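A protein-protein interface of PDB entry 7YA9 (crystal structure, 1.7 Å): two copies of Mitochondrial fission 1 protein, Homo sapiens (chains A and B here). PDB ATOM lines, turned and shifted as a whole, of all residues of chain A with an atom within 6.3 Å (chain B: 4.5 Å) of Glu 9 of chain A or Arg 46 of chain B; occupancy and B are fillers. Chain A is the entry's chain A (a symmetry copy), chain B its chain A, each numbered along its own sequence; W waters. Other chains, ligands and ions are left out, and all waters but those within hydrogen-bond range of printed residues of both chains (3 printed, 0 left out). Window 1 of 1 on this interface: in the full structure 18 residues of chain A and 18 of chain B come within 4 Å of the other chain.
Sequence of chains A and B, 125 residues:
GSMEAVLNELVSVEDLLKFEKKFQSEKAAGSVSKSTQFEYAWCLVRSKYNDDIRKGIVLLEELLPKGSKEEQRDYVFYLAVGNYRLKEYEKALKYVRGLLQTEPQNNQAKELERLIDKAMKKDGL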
ATOM      1  N   GLU A   4       1.963  18.279  18.370  1.00  0.00           N
ATOM      2  CA  GLU A   4       2.921  17.235  18.712  1.00  0.00           C
ATOM      3  C   GLU A   4       4.205  17.840  19.252  1.00  0.00           C
ATOM      4  O   GLU A   4       4.837  17.285  20.167  1.00  0.00           O
ATOM      5  CB  GLU A   4       3.253  16.354  17.480  1.00  0.00           C
ATOM      6  CG  GLU A   4       4.368  15.228  17.695  1.00  0.00           C
ATOM      7  CD  GLU A   4       5.886  15.660  17.685  1.00  0.00           C
ATOM      8  OE1 GLU A   4       6.339  16.658  17.024  1.00  0.00           O
ATOM      9  OE2 GLU A   4       6.671  14.938  18.348  1.00  0.00           O
ATOM     10  N   ALA A   5       4.650  18.930  18.655  1.00  0.00           N
ATOM     11  CA  ALA A   5       5.890  19.548  19.099  1.00  0.00           C
ATOM     12  C   ALA A   5       5.762  20.046  20.531  1.00  0.00           C
ATOM     13  O   ALA A   5       6.677  19.861  21.348  1.00  0.00           O
ATOM     14  CB  ALA A   5       6.283  20.679  18.145  1.00  0.00           C
ATOM     15  N   VAL A   6       4.632  20.667  20.853  1.00  0.00           N
ATOM     16  CA  VAL A   6       4.415  21.192  22.203  1.00  0.00           C
ATOM     17  C   VAL A   6       4.287  20.042  23.204  1.00  0.00           C
ATOM     18  O   VAL A   6       4.880  20.072  24.293  1.00  0.00           O
ATOM     19  CB  VAL A   6       3.163  22.077  22.184  1.00  0.00           C
ATOM     20  CG1 VAL A   6       2.688  22.357  23.602  1.00  0.00           C
ATOM     21  CG2 VAL A   6       3.523  23.370  21.414  1.00  0.00           C
ATOM     22  N   LEU A   7       3.551  18.997  22.839  1.00  0.00           N
ATOM     23  CA  LEU A   7       3.345  17.850  23.727  1.00  0.00           C
ATOM     24  C   LEU A   7       4.643  17.137  24.102  1.00  0.00           C
ATOM     25  O   LEU A   7       4.802  16.713  25.273  1.00  0.00           O
ATOM     26  CB  LEU A   7       2.388  16.832  23.089  1.00  0.00           C
ATOM     27  CG  LEU A   7       2.058  15.596  23.961  1.00  0.00           C
ATOM     28  CD1 LEU A   7       1.364  15.903  25.301  1.00  0.00           C
ATOM     29  CD2 LEU A   7       1.065  14.655  23.156  1.00  0.00           C
ATOM     30  N   ASN A   8       5.597  17.041  23.169  1.00  0.00           N
ATOM     31  CA  ASN A   8       6.839  16.278  23.368  1.00  0.00           C
ATOM     32  C   ASN A   8       8.044  17.157  23.676  1.00  0.00           C
ATOM     33  O   ASN A   8       9.165  16.644  23.761  1.00  0.00           O
ATOM     34  CB  ASN A   8       7.129  15.420  22.123  1.00  0.00           C
ATOM     35  CG  ASN A   8       6.081  14.344  21.964  1.00  0.00           C
ATOM     36  OD1 ASN A   8       5.387  14.237  20.936  1.00  0.00           O
ATOM     37  ND2 ASN A   8       5.906  13.590  23.009  1.00  0.00           N
ATOM     38  N   GLU A   9       7.821  18.457  23.902  1.00  0.00           N
ATOM     39  CA  GLU A   9       8.938  19.377  24.070  1.00  0.00           C
ATOM     40  C   GLU A   9       9.715  19.071  25.343  1.00  0.00           C
ATOM     41  O   GLU A   9       9.116  18.830  26.394  1.00  0.00           O
ATOM     42  CB  GLU A   9       8.423  20.829  24.172  1.00  0.00           C
ATOM     43  CG  GLU A   9       9.694  21.743  23.971  1.00  0.00           C
ATOM     44  CD  GLU A   9       9.436  23.227  23.830  1.00  0.00           C
ATOM     45  OE1 GLU A   9       8.368  23.632  24.295  1.00  0.00           O
ATOM     46  OE2 GLU A   9      10.369  23.949  23.313  1.00  0.00           O
ATOM     47  N   LEU A  10      11.033  19.152  25.272  1.00  0.00           N
ATOM     48  CA  LEU A  10      11.840  19.012  26.472  1.00  0.00           C
ATOM     49  C   LEU A  10      12.314  20.407  26.871  1.00  0.00           C
ATOM     50  O   LEU A  10      12.908  21.112  26.040  1.00  0.00           O
ATOM     51  CB  LEU A  10      13.062  18.099  26.211  1.00  0.00           C
ATOM     52  CG  LEU A  10      12.667  16.614  26.026  1.00  0.00           C
ATOM     53  CD1 LEU A  10      13.817  15.802  25.466  1.00  0.00           C
ATOM     54  CD2 LEU A  10      12.265  16.094  27.362  1.00  0.00           C
ATOM     55  N   VAL A  11      12.120  20.787  28.149  1.00  0.00           N
ATOM     56  CA  VAL A  11      12.631  22.074  28.587  1.00  0.00           C
ATOM     57  C   VAL A  11      14.166  22.062  28.612  1.00  0.00           C
ATOM     58  O   VAL A  11      14.805  21.012  28.836  1.00  0.00           O
ATOM     59  CB  VAL A  11      12.060  22.384  29.981  1.00  0.00           C
ATOM     60  CG1 VAL A  11      12.595  21.377  31.022  1.00  0.00           C
ATOM     61  CG2 VAL A  11      12.354  23.856  30.418  1.00  0.00           C
ATOM     62  N   TRP A  42       5.425  24.439  34.681  1.00  0.00           N
ATOM     63  CA  TRP A  42       5.485  24.334  33.206  1.00  0.00           C
ATOM     64  C   TRP A  42       6.823  23.765  32.744  1.00  0.00           C
ATOM     65  O   TRP A  42       6.882  23.005  31.755  1.00  0.00           O
ATOM     66  CB  TRP A  42       5.270  25.760  32.636  1.00  0.00           C
ATOM     67  CG  TRP A  42       5.562  25.965  31.198  1.00  0.00           C
ATOM     68  CD1 TRP A  42       4.893  25.399  30.120  1.00  0.00           C
ATOM     69  CD2 TRP A  42       6.543  26.869  30.668  1.00  0.00           C
ATOM     70  NE1 TRP A  42       5.441  25.918  28.925  1.00  0.00           N
ATOM     71  CE2 TRP A  42       6.448  26.805  29.242  1.00  0.00           C
ATOM     72  CE3 TRP A  42       7.502  27.753  31.276  1.00  0.00           C
ATOM     73  CZ2 TRP A  42       7.267  27.575  28.401  1.00  0.00           C
ATOM     74  CZ3 TRP A  42       8.311  28.523  30.451  1.00  0.00           C
ATOM     75  CH2 TRP A  42       8.193  28.425  29.014  1.00  0.00           C
ATOM     76  N   VAL A  45       6.961  19.767  34.067  1.00  0.00           N
ATOM     77  CA  VAL A  45       6.210  18.734  33.344  1.00  0.00           C
ATOM     78  C   VAL A  45       6.804  18.516  31.961  1.00  0.00           C
ATOM     79  O   VAL A  45       6.407  17.520  31.297  1.00  0.00           O
ATOM     80  CB  VAL A  45       4.696  18.998  33.201  1.00  0.00           C
ATOM     81  CG1 VAL A  45       3.984  19.107  34.588  1.00  0.00           C
ATOM     82  CG2 VAL A  45       4.390  20.300  32.376  1.00  0.00           C
ATOM     83  N   ARG A  46       7.683  19.425  31.480  1.00  0.00           N
ATOM     84  CA  ARG A  46       8.402  19.224  30.218  1.00  0.00           C
ATOM     85  C   ARG A  46       9.798  18.659  30.437  1.00  0.00           C
ATOM     86  O   ARG A  46      10.622  18.671  29.531  1.00  0.00           O
ATOM     87  CB  ARG A  46       8.460  20.549  29.417  1.00  0.00           C
ATOM     88  CG  ARG A  46       7.023  21.010  29.020  1.00  0.00           C
ATOM     89  CD  ARG A  46       7.033  22.421  28.333  1.00  0.00           C
ATOM     90  NE  ARG A  46       7.741  23.430  29.128  1.00  0.00           N
ATOM     91  CZ  ARG A  46       8.635  24.272  28.679  1.00  0.00           C
ATOM     92  NH1 ARG A  46       8.881  24.383  27.356  1.00  0.00           N
ATOM     93  NH2 ARG A  46       9.205  25.132  29.522  1.00  0.00           N
ATOM     94  N   SER A  47      10.105  18.198  31.648  1.00  0.00           N
ATOM     95  CA  SER A  47      11.438  17.636  31.906  1.00  0.00           C
ATOM     96  C   SER A  47      11.573  16.237  31.301  1.00  0.00           C
ATOM     97  O   SER A  47      10.579  15.583  31.040  1.00  0.00           O
ATOM     98  CB  SER A  47      11.647  17.480  33.436  1.00  0.00           C
ATOM     99  OG  SER A  47      12.979  17.010  33.726  1.00  0.00           O
ATOM    100  N   ARG A  85       3.306  12.331  29.805  1.00  0.00           N
ATOM    101  CA  ARG A  85       4.724  12.035  29.861  1.00  0.00           C
ATOM    102  C   ARG A  85       5.037  10.900  30.838  1.00  0.00           C
ATOM    103  O   ARG A  85       6.056  10.238  30.661  1.00  0.00           O
ATOM    104  CB  ARG A  85       5.510  13.316  30.259  1.00  0.00           C
ATOM    105  CG  ARG A  85       5.226  14.613  29.374  1.00  0.00           C
ATOM    106  CD  ARG A  85       5.891  14.585  28.015  1.00  0.00           C
ATOM    107  NE  ARG A  85       7.234  15.035  28.245  1.00  0.00           N
ATOM    108  CZ  ARG A  85       7.749  16.194  27.847  1.00  0.00           C
ATOM    109  NH1 ARG A  85       7.059  17.058  27.089  1.00  0.00           N
ATOM    110  NH2 ARG A  85       8.991  16.402  28.204  1.00  0.00           N
ATOM    111  N   GLU B   9      12.799  32.417  26.435  1.00  0.00           N
ATOM    112  CA  GLU B   9      12.985  30.978  26.566  1.00  0.00           C
ATOM    113  C   GLU B   9      14.175  30.501  25.744  1.00  0.00           C
ATOM    114  O   GLU B   9      14.341  30.914  24.594  1.00  0.00           O
ATOM    115  CB  GLU B   9      11.733  30.230  26.058  1.00  0.00           C
ATOM    116  CG  GLU B   9      11.884  28.750  26.585  1.00  0.00           C
ATOM    117  CD  GLU B   9      10.687  27.845  26.393  1.00  0.00           C
ATOM    118  OE1 GLU B   9       9.901  28.178  25.502  1.00  0.00           O
ATOM    119  OE2 GLU B   9      10.624  26.776  27.109  1.00  0.00           O
ATOM    120  N   LEU B  10      14.953  29.585  26.295  1.00  0.00           N
ATOM    121  CA  LEU B  10      16.025  28.977  25.527  1.00  0.00           C
ATOM    122  C   LEU B  10      15.567  27.575  25.132  1.00  0.00           C
ATOM    123  O   LEU B  10      15.176  26.789  26.009  1.00  0.00           O
ATOM    124  CB  LEU B  10      17.322  28.887  26.366  1.00  0.00           C
ATOM    125  CG  LEU B  10      17.971  30.271  26.609  1.00  0.00           C
ATOM    126  CD1 LEU B  10      19.042  30.198  27.679  1.00  0.00           C
ATOM    127  CD2 LEU B  10      18.557  30.717  25.315  1.00  0.00           C
ATOM    128  N   VAL B  11      15.676  27.230  23.833  1.00  0.00           N
ATOM    129  CA  VAL B  11      15.328  25.878  23.433  1.00  0.00           C
ATOM    130  C   VAL B  11      16.345  24.873  23.994  1.00  0.00           C
ATOM    131  O   VAL B  11      17.536  25.194  24.190  1.00  0.00           O
ATOM    132  CB  VAL B  11      15.280  25.814  21.898  1.00  0.00           C
ATOM    133  CG1 VAL B  11      16.685  26.048  21.301  1.00  0.00           C
ATOM    134  CG2 VAL B  11      14.669  24.468  21.388  1.00  0.00           C
ATOM    135  N   ASP B  15      15.554  19.339  21.545  1.00  0.00           N
ATOM    136  CA  ASP B  15      14.559  19.775  20.563  1.00  0.00           C
ATOM    137  C   ASP B  15      15.198  20.443  19.358  1.00  0.00           C
ATOM    138  O   ASP B  15      14.774  20.211  18.224  1.00  0.00           O
ATOM    139  CB  ASP B  15      13.546  20.690  21.222  1.00  0.00           C
ATOM    140  CG  ASP B  15      12.481  19.882  21.986  1.00  0.00           C
ATOM    141  OD1 ASP B  15      11.781  19.016  21.382  1.00  0.00           O
ATOM    142  OD2 ASP B  15      12.359  20.117  23.181  1.00  0.00           O
ATOM    143  N   TRP B  42      11.390  27.950  14.782  1.00  0.00           N
ATOM    144  CA  TRP B  42      10.938  28.211  16.167  1.00  0.00           C
ATOM    145  C   TRP B  42      12.008  27.821  17.182  1.00  0.00           C
ATOM    146  O   TRP B  42      12.172  28.492  18.223  1.00  0.00           O
ATOM    147  CB  TRP B  42       9.644  27.385  16.391  1.00  0.00           C
ATOM    148  CG  TRP B  42       9.156  27.259  17.784  1.00  0.00           C
ATOM    149  CD1 TRP B  42       8.683  28.280  18.600  1.00  0.00           C
ATOM    150  CD2 TRP B  42       8.999  26.027  18.503  1.00  0.00           C
ATOM    151  NE1 TRP B  42       8.246  27.716  19.820  1.00  0.00           N
ATOM    152  CE2 TRP B  42       8.439  26.352  19.779  1.00  0.00           C
ATOM    153  CE3 TRP B  42       9.273  24.652  18.178  1.00  0.00           C
ATOM    154  CZ2 TRP B  42       8.147  25.371  20.741  1.00  0.00           C
ATOM    155  CZ3 TRP B  42       8.981  23.676  19.122  1.00  0.00           C
ATOM    156  CH2 TRP B  42       8.424  24.043  20.404  1.00  0.00           C
ATOM    157  N   CYS B  43      12.724  26.714  16.926  1.00  0.00           N
ATOM    158  CA  CYS B  43      13.841  26.360  17.788  1.00  0.00           C
ATOM    159  C   CYS B  43      15.014  27.322  17.595  1.00  0.00           C
ATOM    160  O   CYS B  43      15.639  27.755  18.590  1.00  0.00           O
ATOM    161  CB  CYS B  43      14.331  24.947  17.500  1.00  0.00           C
ATOM    162  SG  CYS B  43      13.027  23.696  17.976  1.00  0.00           S
ATOM    163  N   LEU B  44      15.329  27.643  16.345  1.00  0.00           N
ATOM    164  CA  LEU B  44      16.510  28.481  16.045  1.00  0.00           C
ATOM    165  C   LEU B  44      16.409  29.858  16.694  1.00  0.00           C
ATOM    166  O   LEU B  44      17.396  30.343  17.273  1.00  0.00           O
ATOM    167  CB  LEU B  44      16.697  28.650  14.526  1.00  0.00           C
ATOM    168  CG  LEU B  44      17.228  27.342  13.848  1.00  0.00           C
ATOM    169  CD1 LEU B  44      17.053  27.498  12.300  1.00  0.00           C
ATOM    170  CD2 LEU B  44      18.720  27.123  14.168  1.00  0.00           C
ATOM    171  N   VAL B  45      15.229  30.481  16.630  1.00  0.00           N
ATOM    172  CA  VAL B  45      15.145  31.847  17.161  1.00  0.00           C
ATOM    173  C   VAL B  45      15.151  31.826  18.682  1.00  0.00           C
ATOM    174  O   VAL B  45      15.296  32.922  19.288  1.00  0.00           O
ATOM    175  CB  VAL B  45      13.931  32.669  16.678  1.00  0.00           C
ATOM    176  CG1 VAL B  45      13.922  32.848  15.125  1.00  0.00           C
ATOM    177  CG2 VAL B  45      12.563  32.033  17.119  1.00  0.00           C
ATOM    178  N   ARG B  46      14.944  30.649  19.317  1.00  0.00           N
ATOM    179  CA  ARG B  46      15.066  30.516  20.772  1.00  0.00           C
ATOM    180  C   ARG B  46      16.430  29.982  21.186  1.00  0.00           C
ATOM    181  O   ARG B  46      16.615  29.568  22.323  1.00  0.00           O
ATOM    182  CB  ARG B  46      13.929  29.620  21.325  1.00  0.00           C
ATOM    183  CG  ARG B  46      12.540  30.285  21.074  1.00  0.00           C
ATOM    184  CD  ARG B  46      11.358  29.340  21.492  1.00  0.00           C
ATOM    185  NE  ARG B  46      11.457  28.010  20.882  1.00  0.00           N
ATOM    186  CZ  ARG B  46      11.315  26.869  21.504  1.00  0.00           C
ATOM    187  NH1 ARG B  46      10.901  26.824  22.788  1.00  0.00           N
ATOM    188  NH2 ARG B  46      11.440  25.731  20.820  1.00  0.00           N
ATOM    189  N   SER B  47      17.391  29.938  20.266  1.00  0.00           N
ATOM    190  CA  SER B  47      18.727  29.437  20.620  1.00  0.00           C
ATOM    191  C   SER B  47      19.505  30.472  21.435  1.00  0.00           C
ATOM    192  O   SER B  47      19.189  31.648  21.395  1.00  0.00           O
ATOM    193  CB  SER B  47      19.545  29.184  19.326  1.00  0.00           C
ATOM    194  OG  SER B  47      20.831  28.611  19.637  1.00  0.00           O
ATOM    195  N   LYS B  48      20.509  30.003  22.163  1.00  0.00           N
ATOM    196  CA  LYS B  48      21.443  30.936  22.800  1.00  0.00           C
ATOM    197  C   LYS B  48      22.431  31.545  21.816  1.00  0.00           C
ATOM    198  O   LYS B  48      23.088  32.538  22.159  1.00  0.00           O
ATOM    199  CB  LYS B  48      22.302  30.291  23.900  1.00  0.00           C
ATOM    200  CG  LYS B  48      21.925  29.025  24.485  1.00  0.00           C
ATOM    201  CD  LYS B  48      23.158  28.416  25.184  1.00  0.00           C
ATOM    202  CE  LYS B  48      22.877  28.034  26.626  1.00  0.00           C
ATOM    203  NZ  LYS B  48      22.965  29.163  27.615  1.00  0.00           N
ATOM    204  N   ARG B  85      16.123  39.017  20.258  1.00  0.00           N
ATOM    205  CA  ARG B  85      17.263  38.295  20.789  1.00  0.00           C
ATOM    206  C   ARG B  85      18.582  38.780  20.186  1.00  0.00           C
ATOM    207  O   ARG B  85      19.614  38.624  20.834  1.00  0.00           O
ATOM    208  CB  ARG B  85      17.083  36.773  20.530  1.00  0.00           C
ATOM    209  CG  ARG B  85      15.710  36.135  21.035  1.00  0.00           C
ATOM    210  CD  ARG B  85      15.646  35.923  22.532  1.00  0.00           C
ATOM    211  NE  ARG B  85      16.313  34.673  22.763  1.00  0.00           N
ATOM    212  CZ  ARG B  85      15.734  33.539  23.146  1.00  0.00           C
ATOM    213  NH1 ARG B  85      14.430  33.470  23.447  1.00  0.00           N
ATOM    214  NH2 ARG B  85      16.542  32.515  23.260  1.00  0.00           N
HETATM  215  O   HOH W   1       7.935  26.383  24.623  1.00  0.00           O
HETATM  216  O   HOH W   2      11.451  16.515  22.385  1.00  0.00           O
HETATM  217  O   HOH W   3       9.149  18.761  20.540  1.00  0.00           O
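Of the 12 printed residues of chain B, 4 touch a printed residue of chain A.
Hydrophobic or aromatic side chains of chain B that line the printed part of chain A: Trp 42.
Of the 13 printed residues of chain A, 4 touch a printed residue of chain B.
Hydrophobic or aromatic side chains of chain A within 4 Å of the printed part of chain B: Leu 10 and Trp 42.
Of chain B, only Asp 15 (3.2 Å), Trp 42 (3.5 Å) and Arg 46 (3.0 Å) come within 4 Å of Glu 9 of chain A.
Arg 46 of chain B touches just one residue of chain A: Glu 9.
Of the printed residues of chain A, Trp 42 of chain B touches Glu 9 (3.5 Å).
Printed residues of chain A within 4 Å of Glu 9 of chain B: Trp 42 (3.5 Å) and Arg 46 (3.0 Å).
Of the printed residues of chain B, Trp 42 of chain A touches Glu 9.
Arg 85 of chain B touches none of the printed residues of chain A.
The nearest printed residue of chain B that does not touch Glu 9 of chain A is Val 11 of chain B (4.7 Å).
The nearest printed residue of chain A that does not touch Glu 9 of chain B is Glu 9 of chain A (4.7 Å).
Glu 9 of chain A touches Trp 42 of chain B, and with the chains exchanged Trp 42 of chain A touches Glu 9 of chain B.
Glu 9 of chain A touches Arg 46 of chain B, and with the chains exchanged Arg 46 of chain A touches Glu 9 of chain B.
8 positions are printed for both chains.
Of the 6 pairs that touch across the chains among the printed residues, 4 have their exchanged pair printed and touching as well.
Water W2 bridges O of Asn 8 of chain A (2.7 Å) and OD1 of Asp 15 of chain B (2.7 Å).
Water W3 lies within hydrogen-bond range of the side-chain carboxylate (OD1) of Asp 15 of chain B and the backbone carbonyl oxygen (O) of Ala 5 of chain A.
Water W1 bridges the side-chain carboxylate (OE1) of Glu 9 of chain B and the side-chain carboxylate (OE1) of Glu 9 of chain A.
The side-chain carboxylate (OE2) of Glu 9 of chain B lies within salt-bridge range of the guanidinium group (NH1) of Arg 46 of chain A (3.0 Å).
The side-chain carboxylate (OD2) of Asp 15 of chain B sits at hydrogen-bond distance from the backbone NH (N) of Leu 10 of chain A, at 2.7 Å.
NH1 of Arg 46 of chain B is in salt-bridge range of OE2 of Glu 9 of chain A (3.0 Å).
OD2 of Asp 15 of chain B touches CG of Glu 9 of chain A, 3.2 Å away.
Trp 42 of chain B touches Glu 9 of chain A (CH2 to OE2, 3.5 Å).
OE2 of Glu 9 of chain B touches CH2 of Trp 42 of chain A, at 3.5 Å.
NH1 of Arg 46 of chain B lies within salt-bridge range of OE1 of Glu 9 of chain B (3.2 Å).
The backbone carbonyl oxygen of Glu 9 of chain B is in hydrogen-bond range of the guanidinium group of Arg 85 of chain B (2.8 Å).
The backbone carbonyl oxygen (O) of Trp 42 of chain B sits at hydrogen-bond distance from the guanidinium group (NE) of Arg 46 of chain B.
The side-chain carboxylate (OE1) of Glu 9 of chain A lies within salt-bridge range of the guanidinium group (NH1) of Arg 46 of chain A, at 3.2 Å.
N of Val 11 of chain A is in hydrogen-bond range of O of Arg 46 of chain A, 2.9 Å away.
The backbone carbonyl oxygen (O) of Arg 46 of chain A lies within hydrogen-bond range of the guanidinium group (NH2) of Arg 85 of chain A (3.1 Å).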
